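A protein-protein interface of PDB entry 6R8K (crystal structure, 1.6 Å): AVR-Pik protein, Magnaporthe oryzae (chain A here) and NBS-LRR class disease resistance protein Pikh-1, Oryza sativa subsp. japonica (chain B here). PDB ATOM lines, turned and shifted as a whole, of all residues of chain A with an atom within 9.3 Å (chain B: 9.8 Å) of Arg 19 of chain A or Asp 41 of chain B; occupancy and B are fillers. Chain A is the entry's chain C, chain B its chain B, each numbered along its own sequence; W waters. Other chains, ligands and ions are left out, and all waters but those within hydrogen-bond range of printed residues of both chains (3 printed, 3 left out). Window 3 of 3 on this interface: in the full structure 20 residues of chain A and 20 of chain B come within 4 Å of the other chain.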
ATOM      1  N   ASP A  14       5.256  -3.678  19.696  1.00  0.00           N
ATOM      2  CA  ASP A  14       4.411  -4.130  20.816  1.00  0.00           C
ATOM      3  C   ASP A  14       4.812  -3.338  22.065  1.00  0.00           C
ATOM      4  O   ASP A  14       5.735  -3.759  22.770  1.00  0.00           O
ATOM      5  CB  ASP A  14       4.562  -5.629  20.999  1.00  0.00           C
ATOM      6  CG  ASP A  14       3.709  -6.139  22.141  1.00  0.00           C
ATOM      7  OD1 ASP A  14       3.008  -5.308  22.774  1.00  0.00           O
ATOM      8  OD2 ASP A  14       3.759  -7.354  22.367  1.00  0.00           O
ATOM      9  N   LEU A  15       4.135  -2.245  22.355  1.00  0.00           N
ATOM     10  CA  LEU A  15       4.515  -1.340  23.471  1.00  0.00           C
ATOM     11  C   LEU A  15       4.393  -2.056  24.824  1.00  0.00           C
ATOM     12  O   LEU A  15       5.083  -1.645  25.787  1.00  0.00           O
ATOM     13  CB  LEU A  15       3.631  -0.089  23.446  1.00  0.00           C
ATOM     14  CG  LEU A  15       3.970   0.945  22.375  1.00  0.00           C
ATOM     15  CD1 LEU A  15       3.028   2.146  22.496  1.00  0.00           C
ATOM     16  CD2 LEU A  15       5.421   1.382  22.497  1.00  0.00           C
ATOM     17  N   SER A  16       3.518  -3.062  24.934  1.00  0.00           N
ATOM     18  CA  SER A  16       3.327  -3.819  26.198  1.00  0.00           C
ATOM     19  C   SER A  16       4.622  -4.560  26.552  1.00  0.00           C
ATOM     20  O   SER A  16       4.783  -4.909  27.734  1.00  0.00           O
ATOM     21  CB  SER A  16       2.147  -4.785  26.161  1.00  0.00           C
ATOM     22  OG  SER A  16       2.361  -5.909  25.302  1.00  0.00           O
ATOM     23  N   ARG A  17       5.474  -4.859  25.573  1.00  0.00           N
ATOM     24  CA  ARG A  17       6.715  -5.652  25.785  1.00  0.00           C
ATOM     25  C   ARG A  17       7.946  -4.730  25.797  1.00  0.00           C
ATOM     26  O   ARG A  17       9.092  -5.258  25.753  1.00  0.00           O
ATOM     27  CB  ARG A  17       6.814  -6.745  24.718  1.00  0.00           C
ATOM     28  CG  ARG A  17       5.777  -7.847  24.905  1.00  0.00           C
ATOM     29  CD  ARG A  17       5.875  -9.017  23.939  1.00  0.00           C
ATOM     30  NE  ARG A  17       5.936 -10.279  24.675  1.00  0.00           N
ATOM     31  CZ  ARG A  17       4.947 -11.156  24.785  1.00  0.00           C
ATOM     32  NH1 ARG A  17       5.122 -12.263  25.488  1.00  0.00           N
ATOM     33  NH2 ARG A  17       3.807 -10.956  24.167  1.00  0.00           N
ATOM     34  N   GLU A  18       7.737  -3.425  25.853  1.00  0.00           N
ATOM     35  CA  GLU A  18       8.846  -2.459  25.998  1.00  0.00           C
ATOM     36  C   GLU A  18       9.120  -2.164  27.473  1.00  0.00           C
ATOM     37  O   GLU A  18       8.217  -1.693  28.208  1.00  0.00           O
ATOM     38  CB  GLU A  18       8.555  -1.171  25.224  1.00  0.00           C
ATOM     39  CG  GLU A  18       8.581  -1.321  23.727  1.00  0.00           C
ATOM     40  CD  GLU A  18       9.896  -1.764  23.116  1.00  0.00           C
ATOM     41  OE1 GLU A  18      10.950  -1.630  23.773  1.00  0.00           O
ATOM     42  OE2 GLU A  18       9.865  -2.432  22.022  1.00  0.00           O
ATOM     43  N   ARG A  19      10.338  -2.472  27.905  1.00  0.00           N
ATOM     44  CA  ARG A  19      10.835  -2.113  29.262  1.00  0.00           C
ATOM     45  C   ARG A  19      10.803  -0.611  29.439  1.00  0.00           C
ATOM     46  O   ARG A  19      10.903   0.160  28.461  1.00  0.00           O
ATOM     47  CB  ARG A  19      12.248  -2.653  29.466  1.00  0.00           C
ATOM     48  CG  ARG A  19      13.323  -1.897  28.709  1.00  0.00           C
ATOM     49  CD  ARG A  19      14.657  -2.625  28.748  1.00  0.00           C
ATOM     50  NE  ARG A  19      15.694  -1.953  27.976  1.00  0.00           N
ATOM     51  CZ  ARG A  19      15.881  -2.065  26.660  1.00  0.00           C
ATOM     52  NH1 ARG A  19      15.071  -2.796  25.920  1.00  0.00           N
ATOM     53  NH2 ARG A  19      16.873  -1.432  26.073  1.00  0.00           N
ATOM     54  N   ASP A  20      10.641  -0.184  30.691  1.00  0.00           N
ATOM     55  CA  ASP A  20      10.625   1.258  30.993  1.00  0.00           C
ATOM     56  C   ASP A  20      11.875   1.930  30.458  1.00  0.00           C
ATOM     57  O   ASP A  20      12.988   1.384  30.364  1.00  0.00           O
ATOM     58  CB  ASP A  20      10.509   1.517  32.491  1.00  0.00           C
ATOM     59  CG  ASP A  20       9.183   1.085  33.061  1.00  0.00           C
ATOM     60  OD1 ASP A  20       8.187   0.911  32.284  1.00  0.00           O
ATOM     61  OD2 ASP A  20       9.170   0.868  34.300  1.00  0.00           O
ATOM     62  N   PRO A  21      11.728   3.212  30.128  1.00  0.00           N
ATOM     63  CA  PRO A  21      12.887   4.059  29.905  1.00  0.00           C
ATOM     64  C   PRO A  21      13.723   4.233  31.181  1.00  0.00           C
ATOM     65  O   PRO A  21      13.272   3.915  32.283  1.00  0.00           O
ATOM     66  CB  PRO A  21      12.263   5.413  29.526  1.00  0.00           C
ATOM     67  CG  PRO A  21      10.827   5.103  29.206  1.00  0.00           C
ATOM     68  CD  PRO A  21      10.456   3.923  30.073  1.00  0.00           C
ATOM     69  N   ASN A  22      14.974   4.594  30.964  1.00  0.00           N
ATOM     70  CA  ASN A  22      15.920   5.065  31.998  1.00  0.00           C
ATOM     71  C   ASN A  22      15.723   6.580  32.095  1.00  0.00           C
ATOM     72  O   ASN A  22      16.171   7.264  31.168  1.00  0.00           O
ATOM     73  CB  ASN A  22      17.322   4.604  31.595  1.00  0.00           C
ATOM     74  CG  ASN A  22      18.406   5.075  32.530  1.00  0.00           C
ATOM     75  OD1 ASN A  22      19.493   5.422  32.083  1.00  0.00           O
ATOM     76  ND2 ASN A  22      18.106   5.063  33.814  1.00  0.00           N
ATOM     77  N   PHE A  23      15.045   7.054  33.133  1.00  0.00           N
ATOM     78  CA  PHE A  23      14.602   8.464  33.197  1.00  0.00           C
ATOM     79  C   PHE A  23      14.931   9.046  34.566  1.00  0.00           C
ATOM     80  O   PHE A  23      15.255   8.310  35.513  1.00  0.00           O
ATOM     81  CB  PHE A  23      13.110   8.552  32.890  1.00  0.00           C
ATOM     82  CG  PHE A  23      12.250   7.928  33.952  1.00  0.00           C
ATOM     83  CD1 PHE A  23      12.028   6.561  33.976  1.00  0.00           C
ATOM     84  CD2 PHE A  23      11.657   8.711  34.930  1.00  0.00           C
ATOM     85  CE1 PHE A  23      11.237   5.987  34.960  1.00  0.00           C
ATOM     86  CE2 PHE A  23      10.885   8.132  35.926  1.00  0.00           C
ATOM     87  CZ  PHE A  23      10.672   6.779  35.934  1.00  0.00           C
ATOM     88  N   PHE A  35       5.615   8.148  28.858  1.00  0.00           N
ATOM     89  CA  PHE A  35       6.855   7.551  28.317  1.00  0.00           C
ATOM     90  C   PHE A  35       6.785   7.660  26.793  1.00  0.00           C
ATOM     91  O   PHE A  35       5.706   7.424  26.215  1.00  0.00           O
ATOM     92  CB  PHE A  35       7.016   6.101  28.761  1.00  0.00           C
ATOM     93  CG  PHE A  35       7.306   5.845  30.216  1.00  0.00           C
ATOM     94  CD1 PHE A  35       8.182   6.662  30.928  1.00  0.00           C
ATOM     95  CD2 PHE A  35       6.733   4.764  30.867  1.00  0.00           C
ATOM     96  CE1 PHE A  35       8.488   6.404  32.258  1.00  0.00           C
ATOM     97  CE2 PHE A  35       7.061   4.489  32.185  1.00  0.00           C
ATOM     98  CZ  PHE A  35       7.932   5.301  32.883  1.00  0.00           C
ATOM     99  N   TRP A  36       7.929   7.870  26.141  1.00  0.00           N
ATOM    100  CA  TRP A  36       8.074   7.795  24.679  1.00  0.00           C
ATOM    101  C   TRP A  36       9.116   6.746  24.351  1.00  0.00           C
ATOM    102  O   TRP A  36      10.043   6.527  25.148  1.00  0.00           O
ATOM    103  CB  TRP A  36       8.410   9.150  24.028  1.00  0.00           C
ATOM    104  CG  TRP A  36       9.676   9.773  24.530  1.00  0.00           C
ATOM    105  CD1 TRP A  36       9.800  10.744  25.486  1.00  0.00           C
ATOM    106  CD2 TRP A  36      11.008   9.508  24.049  1.00  0.00           C
ATOM    107  NE1 TRP A  36      11.116  11.054  25.670  1.00  0.00           N
ATOM    108  CE2 TRP A  36      11.875  10.341  24.775  1.00  0.00           C
ATOM    109  CE3 TRP A  36      11.545   8.642  23.089  1.00  0.00           C
ATOM    110  CZ2 TRP A  36      13.250  10.279  24.606  1.00  0.00           C
ATOM    111  CZ3 TRP A  36      12.905   8.613  22.896  1.00  0.00           C
ATOM    112  CH2 TRP A  36      13.748   9.397  23.673  1.00  0.00           C
ATOM    113  N   PHE A  37       8.952   6.155  23.167  1.00  0.00           N
ATOM    114  CA  PHE A  37       9.857   5.099  22.649  1.00  0.00           C
ATOM    115  C   PHE A  37      10.096   5.400  21.176  1.00  0.00           C
ATOM    116  O   PHE A  37       9.115   5.513  20.450  1.00  0.00           O
ATOM    117  CB  PHE A  37       9.226   3.717  22.858  1.00  0.00           C
ATOM    118  CG  PHE A  37       8.807   3.390  24.272  1.00  0.00           C
ATOM    119  CD1 PHE A  37       7.603   3.861  24.772  1.00  0.00           C
ATOM    120  CD2 PHE A  37       9.632   2.652  25.111  1.00  0.00           C
ATOM    121  CE1 PHE A  37       7.230   3.606  26.087  1.00  0.00           C
ATOM    122  CE2 PHE A  37       9.256   2.400  26.424  1.00  0.00           C
ATOM    123  CZ  PHE A  37       8.076   2.888  26.906  1.00  0.00           C
ATOM    124  N   MET A  38      11.355   5.498  20.797  1.00  0.00           N
ATOM    125  CA  MET A  38      11.783   5.859  19.423  1.00  0.00           C
ATOM    126  C   MET A  38      12.250   4.586  18.736  1.00  0.00           C
ATOM    127  O   MET A  38      13.059   3.825  19.350  1.00  0.00           O
ATOM    128  CB  MET A  38      12.912   6.892  19.422  1.00  0.00           C
ATOM    129  CG  MET A  38      13.334   7.218  18.003  1.00  0.00           C
ATOM    130  SD  MET A  38      14.505   8.598  17.948  1.00  0.00           S
ATOM    131  CE  MET A  38      13.646   9.869  18.826  1.00  0.00           C
ATOM    132  N   PHE A  39      11.774   4.335  17.511  1.00  0.00           N
ATOM    133  CA  PHE A  39      12.114   3.131  16.709  1.00  0.00           C
ATOM    134  C   PHE A  39      12.649   3.503  15.337  1.00  0.00           C
ATOM    135  O   PHE A  39      12.165   4.502  14.774  1.00  0.00           O
ATOM    136  CB  PHE A  39      10.921   2.194  16.529  1.00  0.00           C
ATOM    137  CG  PHE A  39      10.325   1.730  17.832  1.00  0.00           C
ATOM    138  CD1 PHE A  39       9.452   2.541  18.553  1.00  0.00           C
ATOM    139  CD2 PHE A  39      10.689   0.515  18.378  1.00  0.00           C
ATOM    140  CE1 PHE A  39       8.924   2.118  19.769  1.00  0.00           C
ATOM    141  CE2 PHE A  39      10.163   0.101  19.589  1.00  0.00           C
ATOM    142  CZ  PHE A  39       9.306   0.908  20.293  1.00  0.00           C
ATOM    143  N   VAL A  43      12.921  -1.235  15.477  1.00  0.00           N
ATOM    144  CA  VAL A  43      13.958  -1.584  16.482  1.00  0.00           C
ATOM    145  C   VAL A  43      14.101  -0.375  17.407  1.00  0.00           C
ATOM    146  O   VAL A  43      14.361   0.735  16.931  1.00  0.00           O
ATOM    147  CB  VAL A  43      15.279  -1.992  15.827  1.00  0.00           C
ATOM    148  CG1 VAL A  43      16.357  -2.297  16.870  1.00  0.00           C
ATOM    149  CG2 VAL A  43      15.072  -3.186  14.915  1.00  0.00           C
ATOM    150  N   ARG A  44      13.923  -0.624  18.696  1.00  0.00           N
ATOM    151  CA  ARG A  44      14.019   0.432  19.733  1.00  0.00           C
ATOM    152  C   ARG A  44      15.399   1.092  19.704  1.00  0.00           C
ATOM    153  O   ARG A  44      16.434   0.353  19.731  1.00  0.00           O
ATOM    154  CB  ARG A  44      13.687  -0.150  21.096  1.00  0.00           C
ATOM    155  CG  ARG A  44      13.951   0.824  22.226  1.00  0.00           C
ATOM    156  CD  ARG A  44      13.432   0.200  23.479  1.00  0.00           C
ATOM    157  NE  ARG A  44      13.756   0.974  24.662  1.00  0.00           N
ATOM    158  CZ  ARG A  44      13.128   0.791  25.812  1.00  0.00           C
ATOM    159  NH1 ARG A  44      12.089  -0.015  25.881  1.00  0.00           N
ATOM    160  NH2 ARG A  44      13.472   1.496  26.870  1.00  0.00           N
ATOM    161  N   GLN A  45      15.416   2.419  19.625  1.00  0.00           N
ATOM    162  CA  GLN A  45      16.650   3.251  19.606  1.00  0.00           C
ATOM    163  C   GLN A  45      16.886   3.873  20.974  1.00  0.00           C
ATOM    164  O   GLN A  45      18.029   3.955  21.406  1.00  0.00           O
ATOM    165  CB  GLN A  45      16.528   4.331  18.531  1.00  0.00           C
ATOM    166  CG  GLN A  45      16.148   3.760  17.177  1.00  0.00           C
ATOM    167  CD  GLN A  45      17.332   3.040  16.595  1.00  0.00           C
ATOM    168  OE1 GLN A  45      18.357   3.665  16.357  1.00  0.00           O
ATOM    169  NE2 GLN A  45      17.201   1.737  16.397  1.00  0.00           N
ATOM    170  N   ASP A  46      15.832   4.394  21.579  1.00  0.00           N
ATOM    171  CA  ASP A  46      15.897   4.975  22.920  1.00  0.00           C
ATOM    172  C   ASP A  46      14.479   5.212  23.388  1.00  0.00           C
ATOM    173  O   ASP A  46      13.521   4.929  22.667  1.00  0.00           O
ATOM    174  CB  ASP A  46      16.700   6.275  22.935  1.00  0.00           C
ATOM    175  CG  ASP A  46      17.350   6.508  24.287  1.00  0.00           C
ATOM    176  OD1 ASP A  46      17.089   5.736  25.205  1.00  0.00           O
ATOM    177  OD2 ASP A  46      18.120   7.454  24.383  1.00  0.00           O
ATOM    178  N   ALA A  47      14.368   5.700  24.614  1.00  0.00           N
ATOM    179  CA  ALA A  47      13.088   5.980  25.247  1.00  0.00           C
ATOM    180  C   ALA A  47      13.291   7.044  26.309  1.00  0.00           C
ATOM    181  O   ALA A  47      14.405   7.204  26.796  1.00  0.00           O
ATOM    182  CB  ALA A  47      12.553   4.729  25.854  1.00  0.00           C
ATOM    183  N   GLY A  48      12.218   7.687  26.705  1.00  0.00           N
ATOM    184  CA  GLY A  48      12.311   8.694  27.774  1.00  0.00           C
ATOM    185  C   GLY A  48      10.946   9.114  28.259  1.00  0.00           C
ATOM    186  O   GLY A  48       9.963   8.400  28.045  1.00  0.00           O
ATOM    187  N   LYS A  88       3.138   6.184  25.715  1.00  0.00           N
ATOM    188  CA  LYS A  88       2.268   5.436  26.655  1.00  0.00           C
ATOM    189  C   LYS A  88       2.124   6.275  27.920  1.00  0.00           C
ATOM    190  O   LYS A  88       3.049   6.983  28.290  1.00  0.00           O
ATOM    191  CB  LYS A  88       2.884   4.072  26.965  1.00  0.00           C
ATOM    192  CG  LYS A  88       2.454   3.441  28.282  1.00  0.00           C
ATOM    193  CD  LYS A  88       2.338   1.927  28.242  1.00  0.00           C
ATOM    194  CE  LYS A  88       3.328   1.257  27.318  1.00  0.00           C
ATOM    195  NZ  LYS A  88       4.693   1.825  27.443  1.00  0.00           N
ATOM    196  N   VAL B   9      18.310  17.887  25.902  1.00  0.00           N
ATOM    197  CA  VAL B   9      19.020  16.586  25.971  1.00  0.00           C
ATOM    198  C   VAL B   9      20.171  16.587  24.968  1.00  0.00           C
ATOM    199  O   VAL B   9      19.930  16.908  23.768  1.00  0.00           O
ATOM    200  CB  VAL B   9      18.093  15.388  25.693  1.00  0.00           C
ATOM    201  CG1 VAL B   9      18.878  14.095  25.772  1.00  0.00           C
ATOM    202  CG2 VAL B   9      16.909  15.346  26.639  1.00  0.00           C
ATOM    203  N   LYS B  11      23.471  14.175  23.573  1.00  0.00           N
ATOM    204  CA  LYS B  11      24.204  12.895  23.504  1.00  0.00           C
ATOM    205  C   LYS B  11      25.685  13.238  23.539  1.00  0.00           C
ATOM    206  O   LYS B  11      26.105  14.133  22.778  1.00  0.00           O
ATOM    207  CB  LYS B  11      23.873  12.101  22.243  1.00  0.00           C
ATOM    208  CG  LYS B  11      24.493  10.717  22.210  1.00  0.00           C
ATOM    209  CD  LYS B  11      24.180   9.954  20.953  1.00  0.00           C
ATOM    210  CE  LYS B  11      25.031   8.712  20.798  1.00  0.00           C
ATOM    211  NZ  LYS B  11      25.449   8.524  19.386  1.00  0.00           N
ATOM    212  N   ARG B  20      31.337  10.089  32.400  1.00  0.00           N
ATOM    213  CA  ARG B  20      29.919  10.484  32.604  1.00  0.00           C
ATOM    214  C   ARG B  20      29.841  11.428  33.800  1.00  0.00           C
ATOM    215  O   ARG B  20      29.142  12.445  33.705  1.00  0.00           O
ATOM    216  CB  ARG B  20      29.051   9.260  32.881  1.00  0.00           C
ATOM    217  CG  ARG B  20      28.842   8.368  31.670  1.00  0.00           C
ATOM    218  CD  ARG B  20      28.176   7.099  32.144  1.00  0.00           C
ATOM    219  NE  ARG B  20      27.616   6.411  30.999  1.00  0.00           N
ATOM    220  CZ  ARG B  20      28.016   5.239  30.538  1.00  0.00           C
ATOM    221  NH1 ARG B  20      28.992   4.566  31.135  1.00  0.00           N
ATOM    222  NH2 ARG B  20      27.419   4.743  29.469  1.00  0.00           N
ATOM    223  N   LEU B  38      21.845  11.735  33.874  1.00  0.00           N
ATOM    224  CA  LEU B  38      22.278  10.808  32.820  1.00  0.00           C
ATOM    225  C   LEU B  38      21.133   9.848  32.535  1.00  0.00           C
ATOM    226  O   LEU B  38      20.720   9.124  33.467  1.00  0.00           O
ATOM    227  CB  LEU B  38      23.482  10.028  33.325  1.00  0.00           C
ATOM    228  CG  LEU B  38      24.043   9.071  32.291  1.00  0.00           C
ATOM    229  CD1 LEU B  38      24.949   9.832  31.329  1.00  0.00           C
ATOM    230  CD2 LEU B  38      24.761   7.934  32.988  1.00  0.00           C
ATOM    231  N   VAL B  39      20.671   9.837  31.295  1.00  0.00           N
ATOM    232  CA  VAL B  39      19.453   9.079  30.922  1.00  0.00           C
ATOM    233  C   VAL B  39      19.707   8.326  29.615  1.00  0.00           C
ATOM    234  O   VAL B  39      20.785   8.425  29.023  1.00  0.00           O
ATOM    235  CB  VAL B  39      18.245  10.033  30.823  1.00  0.00           C
ATOM    236  CG1 VAL B  39      18.002  10.768  32.137  1.00  0.00           C
ATOM    237  CG2 VAL B  39      18.429  11.021  29.696  1.00  0.00           C
ATOM    238  N   GLY B  40      18.697   7.583  29.176  1.00  0.00           N
ATOM    239  CA  GLY B  40      18.729   6.870  27.899  1.00  0.00           C
ATOM    240  C   GLY B  40      19.053   5.413  28.121  1.00  0.00           C
ATOM    241  O   GLY B  40      19.639   5.037  29.160  1.00  0.00           O
ATOM    242  N   ASP B  41      18.704   4.614  27.123  1.00  0.00           N
ATOM    243  CA  ASP B  41      18.883   3.152  27.177  1.00  0.00           C
ATOM    244  C   ASP B  41      20.374   2.844  27.333  1.00  0.00           C
ATOM    245  O   ASP B  41      20.670   1.844  27.979  1.00  0.00           O
ATOM    246  CB  ASP B  41      18.289   2.528  25.914  1.00  0.00           C
ATOM    247  CG  ASP B  41      16.765   2.500  25.871  1.00  0.00           C
ATOM    248  OD1 ASP B  41      16.119   2.725  26.941  1.00  0.00           O
ATOM    249  OD2 ASP B  41      16.235   2.156  24.783  1.00  0.00           O
ATOM    250  N   LEU B  42      21.258   3.653  26.750  1.00  0.00           N
ATOM    251  CA  LEU B  42      22.727   3.404  26.802  1.00  0.00           C
ATOM    252  C   LEU B  42      23.397   4.359  27.790  1.00  0.00           C
ATOM    253  O   LEU B  42      24.626   4.330  27.836  1.00  0.00           O
ATOM    254  CB  LEU B  42      23.312   3.562  25.403  1.00  0.00           C
ATOM    255  CG  LEU B  42      22.931   2.453  24.426  1.00  0.00           C
ATOM    256  CD1 LEU B  42      23.679   2.639  23.119  1.00  0.00           C
ATOM    257  CD2 LEU B  42      23.205   1.075  25.013  1.00  0.00           C
ATOM    258  N   ARG B  43      22.620   5.113  28.574  1.00  0.00           N
ATOM    259  CA  ARG B  43      23.174   5.993  29.640  1.00  0.00           C
ATOM    260  C   ARG B  43      24.229   6.888  28.973  1.00  0.00           C
ATOM    261  O   ARG B  43      25.362   6.997  29.507  1.00  0.00           O
ATOM    262  CB  ARG B  43      23.733   5.102  30.756  1.00  0.00           C
ATOM    263  CG  ARG B  43      22.673   4.270  31.460  1.00  0.00           C
ATOM    264  CD  ARG B  43      23.270   3.257  32.419  1.00  0.00           C
ATOM    265  NE  ARG B  43      24.163   3.920  33.365  1.00  0.00           N
ATOM    266  CZ  ARG B  43      25.488   3.737  33.448  1.00  0.00           C
ATOM    267  NH1 ARG B  43      26.176   4.417  34.351  1.00  0.00           N
ATOM    268  NH2 ARG B  43      26.117   2.892  32.641  1.00  0.00           N
ATOM    269  N   ASP B  44      23.901   7.455  27.811  1.00  0.00           N
ATOM    270  CA  ASP B  44      24.810   8.275  26.964  1.00  0.00           C
ATOM    271  C   ASP B  44      24.230   9.663  26.695  1.00  0.00           C
ATOM    272  O   ASP B  44      24.781  10.388  25.837  1.00  0.00           O
ATOM    273  CB  ASP B  44      25.121   7.566  25.647  1.00  0.00           C
ATOM    274  CG  ASP B  44      23.921   7.245  24.772  1.00  0.00           C
ATOM    275  OD1 ASP B  44      22.762   7.399  25.246  1.00  0.00           O
ATOM    276  OD2 ASP B  44      24.158   6.820  23.614  1.00  0.00           O
ATOM    277  N   LYS B  45      23.135  10.006  27.374  1.00  0.00           N
ATOM    278  CA  LYS B  45      22.449  11.294  27.166  1.00  0.00           C
ATOM    279  C   LYS B  45      22.413  12.092  28.464  1.00  0.00           C
ATOM    280  O   LYS B  45      22.071  11.540  29.526  1.00  0.00           O
ATOM    281  CB  LYS B  45      21.051  11.063  26.599  1.00  0.00           C
ATOM    282  CG  LYS B  45      21.166  10.655  25.135  1.00  0.00           C
ATOM    283  CD  LYS B  45      19.984   9.986  24.566  1.00  0.00           C
ATOM    284  CE  LYS B  45      20.338   9.207  23.313  1.00  0.00           C
ATOM    285  NZ  LYS B  45      19.097   8.856  22.582  1.00  0.00           N
ATOM    286  N   ILE B  46      22.773  13.353  28.347  1.00  0.00           N
ATOM    287  CA  ILE B  46      22.688  14.318  29.471  1.00  0.00           C
ATOM    288  C   ILE B  46      21.427  15.149  29.282  1.00  0.00           C
ATOM    289  O   ILE B  46      21.303  15.839  28.285  1.00  0.00           O
ATOM    290  CB  ILE B  46      23.953  15.197  29.554  1.00  0.00           C
ATOM    291  CG1 ILE B  46      25.212  14.330  29.633  1.00  0.00           C
ATOM    292  CG2 ILE B  46      23.846  16.130  30.747  1.00  0.00           C
ATOM    293  CD1 ILE B  46      26.492  15.124  29.666  1.00  0.00           C
ATOM    294  N   LEU B  72      19.813  16.646  20.955  1.00  0.00           N
ATOM    295  CA  LEU B  72      18.787  15.632  20.570  1.00  0.00           C
ATOM    296  C   LEU B  72      17.381  16.075  20.969  1.00  0.00           C
ATOM    297  O   LEU B  72      16.422  15.596  20.337  1.00  0.00           O
ATOM    298  CB  LEU B  72      19.085  14.290  21.213  1.00  0.00           C
ATOM    299  CG  LEU B  72      20.338  13.588  20.679  1.00  0.00           C
ATOM    300  CD1 LEU B  72      20.417  12.197  21.256  1.00  0.00           C
ATOM    301  CD2 LEU B  72      20.340  13.552  19.158  1.00  0.00           C
HETATM  302  O   HOH W   1      20.735   5.980  25.040  1.00  0.00           O
HETATM  303  O   HOH W   2      21.529   6.624  33.748  1.00  0.00           O
HETATM  304  O   HOH W   3      15.507   8.670  28.980  1.00  0.00           O
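OD2 of Asp 41 of chain B is in salt-bridge range of NE of Arg 44 of chain A (2.7 Å).
The side-chain amino group of Lys 45 of chain B lies within salt-bridge range of the side-chain carboxylate of Asp 46 of chain A (2.5 Å).
The backbone carbonyl oxygen (O) of Gly 40 of chain B lies close to the side-chain amide oxygen (OD1) of Asn 22 of chain A (3.0 Å).
The backbone NH (N) of Asp 41 of chain B is in hydrogen-bond range of the side-chain carboxylate (OD1) of Asp 46 of chain A, 2.7 Å away.
OD2 of Asp 41 of chain B lies within salt-bridge range of NH2 of Arg 19 of chain A, 3.9 Å away.
Printed residues of chain B that touch a printed residue of chain A: Val 39, Gly 40, Asp 41, Arg 43 and Lys 45.
Hydrophobic or aromatic side chains of chain B within 4 Å of the printed part of chain A: Val 39.
Among the printed residues, 8 pairs touch across the chains.
Among the printed residues, Asp or Glu carboxylates within 4 Å of a Lys or Arg side-chain nitrogen of the other chain: Arg 19 of chain A with Asp 41 of chain B (3.9 Å), Arg 44 of chain A with Asp 41 of chain B (2.7 Å) and Asp 46 of chain A with Lys 45 of chain B (2.5 Å).
Val 39 of chain B touches Asn 22 of chain A.
OD1 of Asn 22 of chain A touches CG of Arg 43 of chain B (3.4 Å).
Asp 46 of chain A touches Gly 40 of chain B (OD1 to CA, 3.4 Å).
Water W1 lies within hydrogen-bond range of the side-chain carboxylate of Asp 44 of chain B (2.5 Å), the backbone NH of Leu 42 of chain B (2.9 Å), the side-chain carboxylate of Asp 46 of chain A (3.1 Å) and the backbone NH of Asp 41 of chain B (3.2 Å).
Water W2 lies within hydrogen-bond range of the backbone carbonyl oxygen of Leu 38 of chain B and the side-chain amide oxygen of Asn 22 of chain A.
Water W3 lies within hydrogen-bond range of the backbone carbonyl oxygen (O) of Asn 22 of chain A, the backbone carbonyl oxygen (O) of Ala 47 of chain A and the backbone NH (N) of Gly 40 of chain B.
Glu 18 of chain A touches none of the printed residues of chain B.
Of chain B, only Asp 41 (3.9 Å) comes within 4 Å of Arg 19 of chain A.
No residue of chain B comes within 4 Å of Asp 20 of chain A.
Printed residues of chain B within 4 Å of Arg 44 of chain A: Asp 41 (2.7 Å).
Asp 46 of chain A touches just these residues of chain B: Gly 40, Asp 41 and Lys 45.
Of the printed residues of chain A, Val 39 of chain B touches Asn 22 (3.5 Å).
Printed residues of chain A within 4 Å of Lys 45 of chain B: Asp 46 (2.5 Å).
The nearest residue of chain B that does not touch Arg 19 of chain A is Leu 42 of chain B (6.7 Å).
O of Arg 43 of chain B sits at hydrogen-bond distance from NE of Arg 20 of chain B (2.8 Å).
The backbone NH of Val 39 of chain B is in hydrogen-bond range of the backbone carbonyl oxygen of Lys 45 of chain B, 2.8 Å away.
The backbone carbonyl oxygen (O) of Asp 46 of chain A lies within hydrogen-bond range of the backbone NH (N) of Met 38 of chain A, at 2.9 Å.
O of Arg 19 of chain A sits at hydrogen-bond distance from NH1 of Arg 44 of chain A.
O of Val 39 of chain B lies within hydrogen-bond range of N of Asp 44 of chain B, 3.5 Å away.
NH1 of Arg 44 of chain A lies within salt-bridge range of OE1 of Glu 18 of chain A (2.9 Å).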
